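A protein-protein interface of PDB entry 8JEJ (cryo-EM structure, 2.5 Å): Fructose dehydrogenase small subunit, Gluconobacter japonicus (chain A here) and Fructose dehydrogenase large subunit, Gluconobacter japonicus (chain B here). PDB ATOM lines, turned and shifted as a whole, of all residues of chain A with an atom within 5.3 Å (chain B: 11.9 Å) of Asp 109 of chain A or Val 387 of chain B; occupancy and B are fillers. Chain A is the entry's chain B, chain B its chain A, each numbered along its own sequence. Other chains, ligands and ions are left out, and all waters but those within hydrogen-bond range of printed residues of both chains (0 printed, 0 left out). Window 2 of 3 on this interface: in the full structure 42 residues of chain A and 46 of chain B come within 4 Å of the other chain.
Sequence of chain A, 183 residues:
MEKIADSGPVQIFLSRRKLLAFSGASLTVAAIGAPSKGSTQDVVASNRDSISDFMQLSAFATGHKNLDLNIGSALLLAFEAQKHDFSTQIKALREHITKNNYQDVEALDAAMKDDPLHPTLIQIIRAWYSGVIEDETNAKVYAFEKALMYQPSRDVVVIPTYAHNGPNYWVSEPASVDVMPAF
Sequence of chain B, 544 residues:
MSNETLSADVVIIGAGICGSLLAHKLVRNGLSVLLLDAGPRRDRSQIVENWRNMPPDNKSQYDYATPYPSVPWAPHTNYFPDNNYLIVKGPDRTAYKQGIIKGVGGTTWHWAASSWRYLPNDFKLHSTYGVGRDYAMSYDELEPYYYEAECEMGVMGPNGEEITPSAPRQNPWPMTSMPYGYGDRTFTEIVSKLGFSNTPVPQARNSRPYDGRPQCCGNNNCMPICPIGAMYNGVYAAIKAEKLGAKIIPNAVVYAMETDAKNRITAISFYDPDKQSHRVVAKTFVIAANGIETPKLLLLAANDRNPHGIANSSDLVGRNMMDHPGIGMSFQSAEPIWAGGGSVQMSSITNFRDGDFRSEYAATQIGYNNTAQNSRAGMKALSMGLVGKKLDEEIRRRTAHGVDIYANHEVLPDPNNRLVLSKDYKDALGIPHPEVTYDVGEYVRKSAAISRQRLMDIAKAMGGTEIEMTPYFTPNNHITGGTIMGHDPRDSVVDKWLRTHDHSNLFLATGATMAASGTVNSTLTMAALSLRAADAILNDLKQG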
ATOM      1  N   ALA A  61      32.902 -12.804  19.193  1.00  0.00           N
ATOM      2  CA  ALA A  61      32.034 -13.875  18.716  1.00  0.00           C
ATOM      3  C   ALA A  61      31.953 -15.020  19.717  1.00  0.00           C
ATOM      4  O   ALA A  61      30.870 -15.563  19.961  1.00  0.00           O
ATOM      5  CB  ALA A  61      32.529 -14.382  17.364  1.00  0.00           C
ATOM      6  N   VAL A 105      27.561 -11.230  21.370  1.00  0.00           N
ATOM      7  CA  VAL A 105      27.351 -12.044  20.181  1.00  0.00           C
ATOM      8  C   VAL A 105      25.917 -12.546  20.088  1.00  0.00           C
ATOM      9  O   VAL A 105      25.462 -12.903  18.996  1.00  0.00           O
ATOM     10  CB  VAL A 105      28.350 -13.219  20.150  1.00  0.00           C
ATOM     11  CG1 VAL A 105      27.990 -14.260  21.192  1.00  0.00           C
ATOM     12  CG2 VAL A 105      28.404 -13.840  18.762  1.00  0.00           C
ATOM     13  N   GLU A 106      25.184 -12.579  21.201  1.00  0.00           N
ATOM     14  CA  GLU A 106      23.788 -13.005  21.156  1.00  0.00           C
ATOM     15  C   GLU A 106      22.960 -12.068  20.286  1.00  0.00           C
ATOM     16  O   GLU A 106      22.211 -12.513  19.409  1.00  0.00           O
ATOM     17  CB  GLU A 106      23.219 -13.072  22.572  1.00  0.00           C
ATOM     18  CG  GLU A 106      23.248 -14.456  23.194  1.00  0.00           C
ATOM     19  CD  GLU A 106      24.462 -14.684  24.072  1.00  0.00           C
ATOM     20  OE1 GLU A 106      25.301 -13.767  24.189  1.00  0.00           O
ATOM     21  OE2 GLU A 106      24.575 -15.784  24.650  1.00  0.00           O
ATOM     22  N   ALA A 107      23.094 -10.757  20.508  1.00  0.00           N
ATOM     23  CA  ALA A 107      22.336  -9.788  19.723  1.00  0.00           C
ATOM     24  C   ALA A 107      22.768  -9.795  18.262  1.00  0.00           C
ATOM     25  O   ALA A 107      21.925  -9.705  17.361  1.00  0.00           O
ATOM     26  CB  ALA A 107      22.491  -8.392  20.323  1.00  0.00           C
ATOM     27  N   LEU A 108      24.074  -9.893  18.008  1.00  0.00           N
ATOM     28  CA  LEU A 108      24.558  -9.931  16.632  1.00  0.00           C
ATOM     29  C   LEU A 108      24.035 -11.160  15.901  1.00  0.00           C
ATOM     30  O   LEU A 108      23.611 -11.069  14.743  1.00  0.00           O
ATOM     31  CB  LEU A 108      26.087  -9.901  16.613  1.00  0.00           C
ATOM     32  CG  LEU A 108      26.774 -10.177  15.276  1.00  0.00           C
ATOM     33  CD1 LEU A 108      26.857  -8.911  14.444  1.00  0.00           C
ATOM     34  CD2 LEU A 108      28.159 -10.757  15.501  1.00  0.00           C
ATOM     35  N   ASP A 109      24.049 -12.318  16.564  1.00  0.00           N
ATOM     36  CA  ASP A 109      23.511 -13.531  15.961  1.00  0.00           C
ATOM     37  C   ASP A 109      22.013 -13.409  15.723  1.00  0.00           C
ATOM     38  O   ASP A 109      21.498 -13.879  14.701  1.00  0.00           O
ATOM     39  CB  ASP A 109      23.825 -14.735  16.849  1.00  0.00           C
ATOM     40  CG  ASP A 109      23.020 -15.964  16.475  1.00  0.00           C
ATOM     41  OD1 ASP A 109      23.477 -16.732  15.604  1.00  0.00           O
ATOM     42  OD2 ASP A 109      21.934 -16.165  17.058  1.00  0.00           O
ATOM     43  N   ALA A 110      21.291 -12.783  16.657  1.00  0.00           N
ATOM     44  CA  ALA A 110      19.850 -12.622  16.494  1.00  0.00           C
ATOM     45  C   ALA A 110      19.519 -11.696  15.330  1.00  0.00           C
ATOM     46  O   ALA A 110      18.536 -11.919  14.614  1.00  0.00           O
ATOM     47  CB  ALA A 110      19.232 -12.098  17.789  1.00  0.00           C
ATOM     48  N   ALA A 111      20.317 -10.650  15.128  1.00  0.00           N
ATOM     49  CA  ALA A 111      20.056  -9.660  14.093  1.00  0.00           C
ATOM     50  C   ALA A 111      20.777  -9.958  12.783  1.00  0.00           C
ATOM     51  O   ALA A 111      20.711  -9.147  11.854  1.00  0.00           O
ATOM     52  CB  ALA A 111      20.440  -8.266  14.591  1.00  0.00           C
ATOM     53  N   MET A 112      21.466 -11.097  12.687  1.00  0.00           N
ATOM     54  CA  MET A 112      22.155 -11.492  11.464  1.00  0.00           C
ATOM     55  C   MET A 112      21.734 -12.883  11.009  1.00  0.00           C
ATOM     56  O   MET A 112      22.494 -13.556  10.306  1.00  0.00           O
ATOM     57  CB  MET A 112      23.673 -11.436  11.658  1.00  0.00           C
ATOM     58  CG  MET A 112      24.464 -11.099  10.407  1.00  0.00           C
ATOM     59  SD  MET A 112      26.016 -10.260  10.773  1.00  0.00           S
ATOM     60  CE  MET A 112      25.439  -8.583  11.009  1.00  0.00           C
ATOM     61  N   LYS A 113      20.532 -13.327  11.386  1.00  0.00           N
ATOM     62  CA  LYS A 113      20.121 -14.703  11.126  1.00  0.00           C
ATOM     63  C   LYS A 113      19.960 -15.003   9.642  1.00  0.00           C
ATOM     64  O   LYS A 113      19.922 -16.179   9.265  1.00  0.00           O
ATOM     65  CB  LYS A 113      18.814 -15.006  11.860  1.00  0.00           C
ATOM     66  CG  LYS A 113      18.986 -15.244  13.352  1.00  0.00           C
ATOM     67  CD  LYS A 113      18.083 -16.358  13.851  1.00  0.00           C
ATOM     68  CE  LYS A 113      18.604 -16.945  15.156  1.00  0.00           C
ATOM     69  NZ  LYS A 113      17.786 -18.102  15.614  1.00  0.00           N
ATOM     70  N   HIS A 118      26.427 -14.309   8.336  1.00  0.00           N
ATOM     71  CA  HIS A 118      26.175 -15.286   9.392  1.00  0.00           C
ATOM     72  C   HIS A 118      27.024 -16.546   9.252  1.00  0.00           C
ATOM     73  O   HIS A 118      27.586 -16.998  10.267  1.00  0.00           O
ATOM     74  CB  HIS A 118      24.682 -15.624   9.429  1.00  0.00           C
ATOM     75  CG  HIS A 118      24.193 -16.068  10.772  1.00  0.00           C
ATOM     76  ND1 HIS A 118      23.263 -17.073  10.929  1.00  0.00           N
ATOM     77  CD2 HIS A 118      24.498 -15.639  12.020  1.00  0.00           C
ATOM     78  CE1 HIS A 118      23.019 -17.246  12.216  1.00  0.00           C
ATOM     79  NE2 HIS A 118      23.756 -16.389  12.899  1.00  0.00           N
ATOM     80  N   LEU A 121      30.646 -15.959  10.572  1.00  0.00           N
ATOM     81  CA  LEU A 121      30.674 -15.791  12.023  1.00  0.00           C
ATOM     82  C   LEU A 121      30.502 -17.129  12.734  1.00  0.00           C
ATOM     83  O   LEU A 121      31.232 -17.441  13.689  1.00  0.00           O
ATOM     84  CB  LEU A 121      29.585 -14.807  12.451  1.00  0.00           C
ATOM     85  CG  LEU A 121      29.272 -14.702  13.943  1.00  0.00           C
ATOM     86  CD1 LEU A 121      30.208 -13.714  14.612  1.00  0.00           C
ATOM     87  CD2 LEU A 121      27.822 -14.299  14.155  1.00  0.00           C
ATOM     88  N   ILE A 122      29.546 -17.938  12.271  1.00  0.00           N
ATOM     89  CA  ILE A 122      29.346 -19.260  12.858  1.00  0.00           C
ATOM     90  C   ILE A 122      30.582 -20.126  12.648  1.00  0.00           C
ATOM     91  O   ILE A 122      30.959 -20.917  13.519  1.00  0.00           O
ATOM     92  CB  ILE A 122      28.079 -19.916  12.279  1.00  0.00           C
ATOM     93  CG1 ILE A 122      26.846 -19.078  12.622  1.00  0.00           C
ATOM     94  CG2 ILE A 122      27.911 -21.327  12.812  1.00  0.00           C
ATOM     95  CD1 ILE A 122      26.542 -19.018  14.102  1.00  0.00           C
ATOM     96  N   ILE A 125      33.220 -19.104  15.215  1.00  0.00           N
ATOM     97  CA  ILE A 125      32.874 -19.656  16.525  1.00  0.00           C
ATOM     98  C   ILE A 125      33.178 -21.150  16.569  1.00  0.00           C
ATOM     99  O   ILE A 125      33.752 -21.664  17.541  1.00  0.00           O
ATOM    100  CB  ILE A 125      31.398 -19.372  16.850  1.00  0.00           C
ATOM    101  CG1 ILE A 125      31.191 -17.877  17.085  1.00  0.00           C
ATOM    102  CG2 ILE A 125      30.955 -20.168  18.063  1.00  0.00           C
ATOM    103  CD1 ILE A 125      29.749 -17.463  17.096  1.00  0.00           C
ATOM    104  N   ALA B 377      29.578 -33.682  23.385  1.00  0.00           N
ATOM    105  CA  ALA B 377      28.724 -32.565  23.772  1.00  0.00           C
ATOM    106  C   ALA B 377      29.083 -31.305  23.002  1.00  0.00           C
ATOM    107  O   ALA B 377      28.195 -30.583  22.535  1.00  0.00           O
ATOM    108  CB  ALA B 377      28.834 -32.312  25.273  1.00  0.00           C
ATOM    109  N   GLY B 378      30.379 -31.022  22.862  1.00  0.00           N
ATOM    110  CA  GLY B 378      30.787 -29.837  22.131  1.00  0.00           C
ATOM    111  C   GLY B 378      30.359 -29.878  20.680  1.00  0.00           C
ATOM    112  O   GLY B 378      29.801 -28.910  20.157  1.00  0.00           O
ATOM    113  N   MET B 379      30.596 -31.011  20.011  1.00  0.00           N
ATOM    114  CA  MET B 379      30.203 -31.123  18.609  1.00  0.00           C
ATOM    115  C   MET B 379      28.691 -31.022  18.447  1.00  0.00           C
ATOM    116  O   MET B 379      28.200 -30.330  17.545  1.00  0.00           O
ATOM    117  CB  MET B 379      30.723 -32.432  18.014  1.00  0.00           C
ATOM    118  CG  MET B 379      32.237 -32.581  18.047  1.00  0.00           C
ATOM    119  SD  MET B 379      33.133 -31.127  17.473  1.00  0.00           S
ATOM    120  CE  MET B 379      32.622 -31.074  15.766  1.00  0.00           C
ATOM    121  N   LYS B 380      27.932 -31.695  19.316  1.00  0.00           N
ATOM    122  CA  LYS B 380      26.479 -31.650  19.212  1.00  0.00           C
ATOM    123  C   LYS B 380      25.955 -30.238  19.435  1.00  0.00           C
ATOM    124  O   LYS B 380      25.111 -29.754  18.676  1.00  0.00           O
ATOM    125  CB  LYS B 380      25.849 -32.622  20.208  1.00  0.00           C
ATOM    126  CG  LYS B 380      24.359 -32.417  20.405  1.00  0.00           C
ATOM    127  CD  LYS B 380      23.560 -33.062  19.290  1.00  0.00           C
ATOM    128  CE  LYS B 380      22.069 -32.931  19.541  1.00  0.00           C
ATOM    129  NZ  LYS B 380      21.366 -32.270  18.410  1.00  0.00           N
ATOM    130  N   ALA B 381      26.460 -29.552  20.465  1.00  0.00           N
ATOM    131  CA  ALA B 381      26.000 -28.198  20.752  1.00  0.00           C
ATOM    132  C   ALA B 381      26.392 -27.226  19.651  1.00  0.00           C
ATOM    133  O   ALA B 381      25.652 -26.276  19.376  1.00  0.00           O
ATOM    134  CB  ALA B 381      26.550 -27.729  22.096  1.00  0.00           C
ATOM    135  N   LEU B 382      27.550 -27.434  19.019  1.00  0.00           N
ATOM    136  CA  LEU B 382      27.898 -26.630  17.854  1.00  0.00           C
ATOM    137  C   LEU B 382      26.956 -26.908  16.691  1.00  0.00           C
ATOM    138  O   LEU B 382      26.663 -26.003  15.903  1.00  0.00           O
ATOM    139  CB  LEU B 382      29.345 -26.894  17.440  1.00  0.00           C
ATOM    140  CG  LEU B 382      30.446 -26.270  18.297  1.00  0.00           C
ATOM    141  CD1 LEU B 382      31.800 -26.853  17.925  1.00  0.00           C
ATOM    142  CD2 LEU B 382      30.453 -24.757  18.153  1.00  0.00           C
ATOM    143  N   SER B 383      26.472 -28.147  16.570  1.00  0.00           N
ATOM    144  CA  SER B 383      25.565 -28.485  15.480  1.00  0.00           C
ATOM    145  C   SER B 383      24.186 -27.851  15.635  1.00  0.00           C
ATOM    146  O   SER B 383      23.439 -27.785  14.653  1.00  0.00           O
ATOM    147  CB  SER B 383      25.428 -30.004  15.367  1.00  0.00           C
ATOM    148  OG  SER B 383      24.290 -30.466  16.072  1.00  0.00           O
ATOM    149  N   MET B 384      23.829 -27.385  16.831  1.00  0.00           N
ATOM    150  CA  MET B 384      22.523 -26.782  17.070  1.00  0.00           C
ATOM    151  C   MET B 384      22.476 -25.297  16.735  1.00  0.00           C
ATOM    152  O   MET B 384      21.413 -24.683  16.863  1.00  0.00           O
ATOM    153  CB  MET B 384      22.101 -26.979  18.530  1.00  0.00           C
ATOM    154  CG  MET B 384      22.504 -28.312  19.122  1.00  0.00           C
ATOM    155  SD  MET B 384      21.848 -28.598  20.773  1.00  0.00           S
ATOM    156  CE  MET B 384      20.288 -27.735  20.667  1.00  0.00           C
ATOM    157  N   GLY B 385      23.590 -24.710  16.312  1.00  0.00           N
ATOM    158  CA  GLY B 385      23.619 -23.291  16.002  1.00  0.00           C
ATOM    159  C   GLY B 385      23.432 -22.387  17.202  1.00  0.00           C
ATOM    160  O   GLY B 385      22.774 -21.346  17.090  1.00  0.00           O
ATOM    161  N   LEU B 386      23.995 -22.759  18.346  1.00  0.00           N
ATOM    162  CA  LEU B 386      23.914 -21.947  19.549  1.00  0.00           C
ATOM    163  C   LEU B 386      25.095 -20.987  19.624  1.00  0.00           C
ATOM    164  O   LEU B 386      26.136 -21.190  18.996  1.00  0.00           O
ATOM    165  CB  LEU B 386      23.866 -22.831  20.793  1.00  0.00           C
ATOM    166  CG  LEU B 386      22.508 -23.485  21.038  1.00  0.00           C
ATOM    167  CD1 LEU B 386      22.650 -24.655  21.982  1.00  0.00           C
ATOM    168  CD2 LEU B 386      21.521 -22.472  21.584  1.00  0.00           C
ATOM    169  N   VAL B 387      24.921 -19.929  20.410  1.00  0.00           N
ATOM    170  CA  VAL B 387      25.858 -18.813  20.408  1.00  0.00           C
ATOM    171  C   VAL B 387      25.972 -18.257  21.821  1.00  0.00           C
ATOM    172  O   VAL B 387      25.000 -18.250  22.580  1.00  0.00           O
ATOM    173  CB  VAL B 387      25.410 -17.734  19.392  1.00  0.00           C
ATOM    174  CG1 VAL B 387      25.203 -16.381  20.061  1.00  0.00           C
ATOM    175  CG2 VAL B 387      26.400 -17.634  18.252  1.00  0.00           C
ATOM    176  N   GLY B 388      27.177 -17.813  22.176  1.00  0.00           N
ATOM    177  CA  GLY B 388      27.359 -17.071  23.414  1.00  0.00           C
ATOM    178  C   GLY B 388      27.248 -17.945  24.648  1.00  0.00           C
ATOM    179  O   GLY B 388      27.805 -19.045  24.720  1.00  0.00           O
ATOM    180  N   LYS B 389      26.524 -17.436  25.649  1.00  0.00           N
ATOM    181  CA  LYS B 389      26.356 -18.171  26.898  1.00  0.00           C
ATOM    182  C   LYS B 389      25.533 -19.436  26.702  1.00  0.00           C
ATOM    183  O   LYS B 389      25.765 -20.437  27.390  1.00  0.00           O
ATOM    184  CB  LYS B 389      25.705 -17.276  27.951  1.00  0.00           C
ATOM    185  CG  LYS B 389      26.194 -15.839  27.934  1.00  0.00           C
ATOM    186  CD  LYS B 389      27.138 -15.564  29.091  1.00  0.00           C
ATOM    187  CE  LYS B 389      26.434 -14.805  30.201  1.00  0.00           C
ATOM    188  NZ  LYS B 389      27.266 -14.726  31.432  1.00  0.00           N
ATOM    189  N   LYS B 390      24.568 -19.406  25.779  1.00  0.00           N
ATOM    190  CA  LYS B 390      23.757 -20.589  25.512  1.00  0.00           C
ATOM    191  C   LYS B 390      24.616 -21.742  25.014  1.00  0.00           C
ATOM    192  O   LYS B 390      24.381 -22.900  25.375  1.00  0.00           O
ATOM    193  CB  LYS B 390      22.664 -20.258  24.498  1.00  0.00           C
ATOM    194  CG  LYS B 390      21.882 -19.000  24.820  1.00  0.00           C
ATOM    195  CD  LYS B 390      20.499 -19.334  25.347  1.00  0.00           C
ATOM    196  CE  LYS B 390      20.437 -19.192  26.858  1.00  0.00           C
ATOM    197  NZ  LYS B 390      19.103 -19.570  27.394  1.00  0.00           N
ATOM    198  N   LEU B 391      25.617 -21.443  24.184  1.00  0.00           N
ATOM    199  CA  LEU B 391      26.510 -22.485  23.685  1.00  0.00           C
ATOM    200  C   LEU B 391      27.264 -23.159  24.826  1.00  0.00           C
ATOM    201  O   LEU B 391      27.328 -24.391  24.901  1.00  0.00           O
ATOM    202  CB  LEU B 391      27.484 -21.883  22.670  1.00  0.00           C
ATOM    203  CG  LEU B 391      28.489 -22.807  21.983  1.00  0.00           C
ATOM    204  CD1 LEU B 391      27.783 -23.911  21.220  1.00  0.00           C
ATOM    205  CD2 LEU B 391      29.379 -22.003  21.054  1.00  0.00           C
ATOM    206  N   ASP B 392      27.835 -22.361  25.734  1.00  0.00           N
ATOM    207  CA  ASP B 392      28.578 -22.927  26.856  1.00  0.00           C
ATOM    208  C   ASP B 392      27.666 -23.718  27.784  1.00  0.00           C
ATOM    209  O   ASP B 392      28.036 -24.800  28.260  1.00  0.00           O
ATOM    210  CB  ASP B 392      29.284 -21.816  27.631  1.00  0.00           C
ATOM    211  CG  ASP B 392      30.259 -21.038  26.777  1.00  0.00           C
ATOM    212  OD1 ASP B 392      30.682 -21.559  25.725  1.00  0.00           O
ATOM    213  OD2 ASP B 392      30.607 -19.902  27.160  1.00  0.00           O
ATOM    214  N   GLU B 393      26.470 -23.190  28.058  1.00  0.00           N
ATOM    215  CA  GLU B 393      25.533 -23.900  28.921  1.00  0.00           C
ATOM    216  C   GLU B 393      25.121 -25.229  28.305  1.00  0.00           C
ATOM    217  O   GLU B 393      25.035 -26.245  29.004  1.00  0.00           O
ATOM    218  CB  GLU B 393      24.309 -23.030  29.196  1.00  0.00           C
ATOM    219  CG  GLU B 393      24.593 -21.831  30.080  1.00  0.00           C
ATOM    220  CD  GLU B 393      23.433 -20.861  30.137  1.00  0.00           C
ATOM    221  OE1 GLU B 393      22.364 -21.177  29.575  1.00  0.00           O
ATOM    222  OE2 GLU B 393      23.590 -19.783  30.744  1.00  0.00           O
ATOM    223  N   GLU B 394      24.870 -25.242  26.994  1.00  0.00           N
ATOM    224  CA  GLU B 394      24.518 -26.485  26.320  1.00  0.00           C
ATOM    225  C   GLU B 394      25.668 -27.481  26.360  1.00  0.00           C
ATOM    226  O   GLU B 394      25.452 -28.671  26.604  1.00  0.00           O
ATOM    227  CB  GLU B 394      24.105 -26.203  24.877  1.00  0.00           C
ATOM    228  CG  GLU B 394      23.442 -27.380  24.188  1.00  0.00           C
ATOM    229  CD  GLU B 394      22.010 -27.582  24.635  1.00  0.00           C
ATOM    230  OE1 GLU B 394      21.388 -26.607  25.102  1.00  0.00           O
ATOM    231  OE2 GLU B 394      21.505 -28.718  24.517  1.00  0.00           O
ATOM    232  N   ILE B 395      26.897 -27.016  26.123  1.00  0.00           N
ATOM    233  CA  ILE B 395      28.042 -27.922  26.161  1.00  0.00           C
ATOM    234  C   ILE B 395      28.171 -28.549  27.543  1.00  0.00           C
ATOM    235  O   ILE B 395      28.334 -29.769  27.679  1.00  0.00           O
ATOM    236  CB  ILE B 395      29.332 -27.186  25.752  1.00  0.00           C
ATOM    237  CG1 ILE B 395      29.267 -26.757  24.288  1.00  0.00           C
ATOM    238  CG2 ILE B 395      30.544 -28.075  25.971  1.00  0.00           C
ATOM    239  CD1 ILE B 395      30.289 -25.712  23.913  1.00  0.00           C
ATOM    240  N   ARG B 396      28.077 -27.724  28.590  1.00  0.00           N
ATOM    241  CA  ARG B 396      28.221 -28.228  29.954  1.00  0.00           C
ATOM    242  C   ARG B 396      27.110 -29.212  30.306  1.00  0.00           C
ATOM    243  O   ARG B 396      27.365 -30.284  30.870  1.00  0.00           O
ATOM    244  CB  ARG B 396      28.237 -27.058  30.938  1.00  0.00           C
ATOM    245  CG  ARG B 396      28.401 -27.467  32.390  1.00  0.00           C
ATOM    246  CD  ARG B 396      28.800 -26.280  33.245  1.00  0.00           C
ATOM    247  NE  ARG B 396      28.843 -26.617  34.661  1.00  0.00           N
ATOM    248  CZ  ARG B 396      29.917 -27.070  35.291  1.00  0.00           C
ATOM    249  NH1 ARG B 396      31.061 -27.263  34.657  1.00  0.00           N
ATOM    250  NH2 ARG B 396      29.842 -27.338  36.592  1.00  0.00           N
ATOM    251  N   ARG B 397      25.864 -28.867  29.971  1.00  0.00           N
ATOM    252  CA  ARG B 397      24.751 -29.753  30.287  1.00  0.00           C
ATOM    253  C   ARG B 397      24.869 -31.076  29.542  1.00  0.00           C
ATOM    254  O   ARG B 397      24.618 -32.144  30.112  1.00  0.00           O
ATOM    255  CB  ARG B 397      23.428 -29.063  29.960  1.00  0.00           C
ATOM    256  CG  ARG B 397      22.207 -29.947  30.115  1.00  0.00           C
ATOM    257  CD  ARG B 397      20.924 -29.132  30.081  1.00  0.00           C
ATOM    258  NE  ARG B 397      20.979 -28.038  29.117  1.00  0.00           N
ATOM    259  CZ  ARG B 397      21.023 -26.753  29.442  1.00  0.00           C
ATOM    260  NH1 ARG B 397      21.029 -26.358  30.706  1.00  0.00           N
ATOM    261  NH2 ARG B 397      21.063 -25.840  28.477  1.00  0.00           N
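OD1 of Asp 109 of chain A is in hydrogen-bond range of NE2 of His 118 of chain A.
Ala 61 of chain A touches none of the printed residues of chain B.
Of the printed residues of chain B, Glu 106 of chain A touches Val 387, Gly 388, Lys 389 and Lys 390.
No residue of chain B comes within 4 Å of Ala 107 of chain A.
Leu 108 of chain A touches none of the printed residues of chain B.
Asp 109 of chain A touches just one residue of chain B: Val 387 (3.9 Å).
No residue of chain B comes within 4 Å of Ala 111 of chain A.
Val 387 of chain B touches just these residues of chain A: Val 105, Glu 106, Asp 109 and Ile 125.
Of the printed residues of chain A, Gly 388 of chain B touches Val 105 and Glu 106.
Of the printed residues of chain A, Leu 391 of chain B touches Ile 125 (3.8 Å).
The nearest residue of chain B that does not touch Asp 109 of chain A is Gly 385 of chain B (4.9 Å).
The backbone NH (N) of Lys 389 of chain B is in hydrogen-bond range of the side-chain carboxylate (OE2) of Glu 106 of chain A.
O of Val 387 of chain B sits close to OE2 of Glu 106 of chain A, 3.2 Å away.
Val 105 of chain A touches Val 387 of chain B (O to CG1, 3.6 Å).
Gly 388 of chain B touches Val 105 of chain A (CA to CG1, 3.6 Å).
Glu 106 of chain A touches Gly 388 of chain B (OE2 to CA, 3.3 Å).
Glu 106 of chain A touches Lys 390 of chain B (OE2 to N, 3.8 Å).
Asp 109 of chain A touches Val 387 of chain B.
Ile 125 of chain A touches Val 387 of chain B (CD1 to CG2, 3.5 Å).
Ile 125 of chain A touches Leu 391 of chain B (CG2 to CD2, 3.8 Å).
Of the 21 printed residues of chain B, 5 touch a printed residue of chain A.
Hydrophobic or aromatic side chains of chain B that line the printed part of chain A: Val 387 and Leu 391.
Among the printed residues, 9 pairs touch across the chains.
Among the printed residues, no Asp or Glu carboxylate lies within 4 Å of a Lys or Arg side-chain nitrogen of the other chain.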
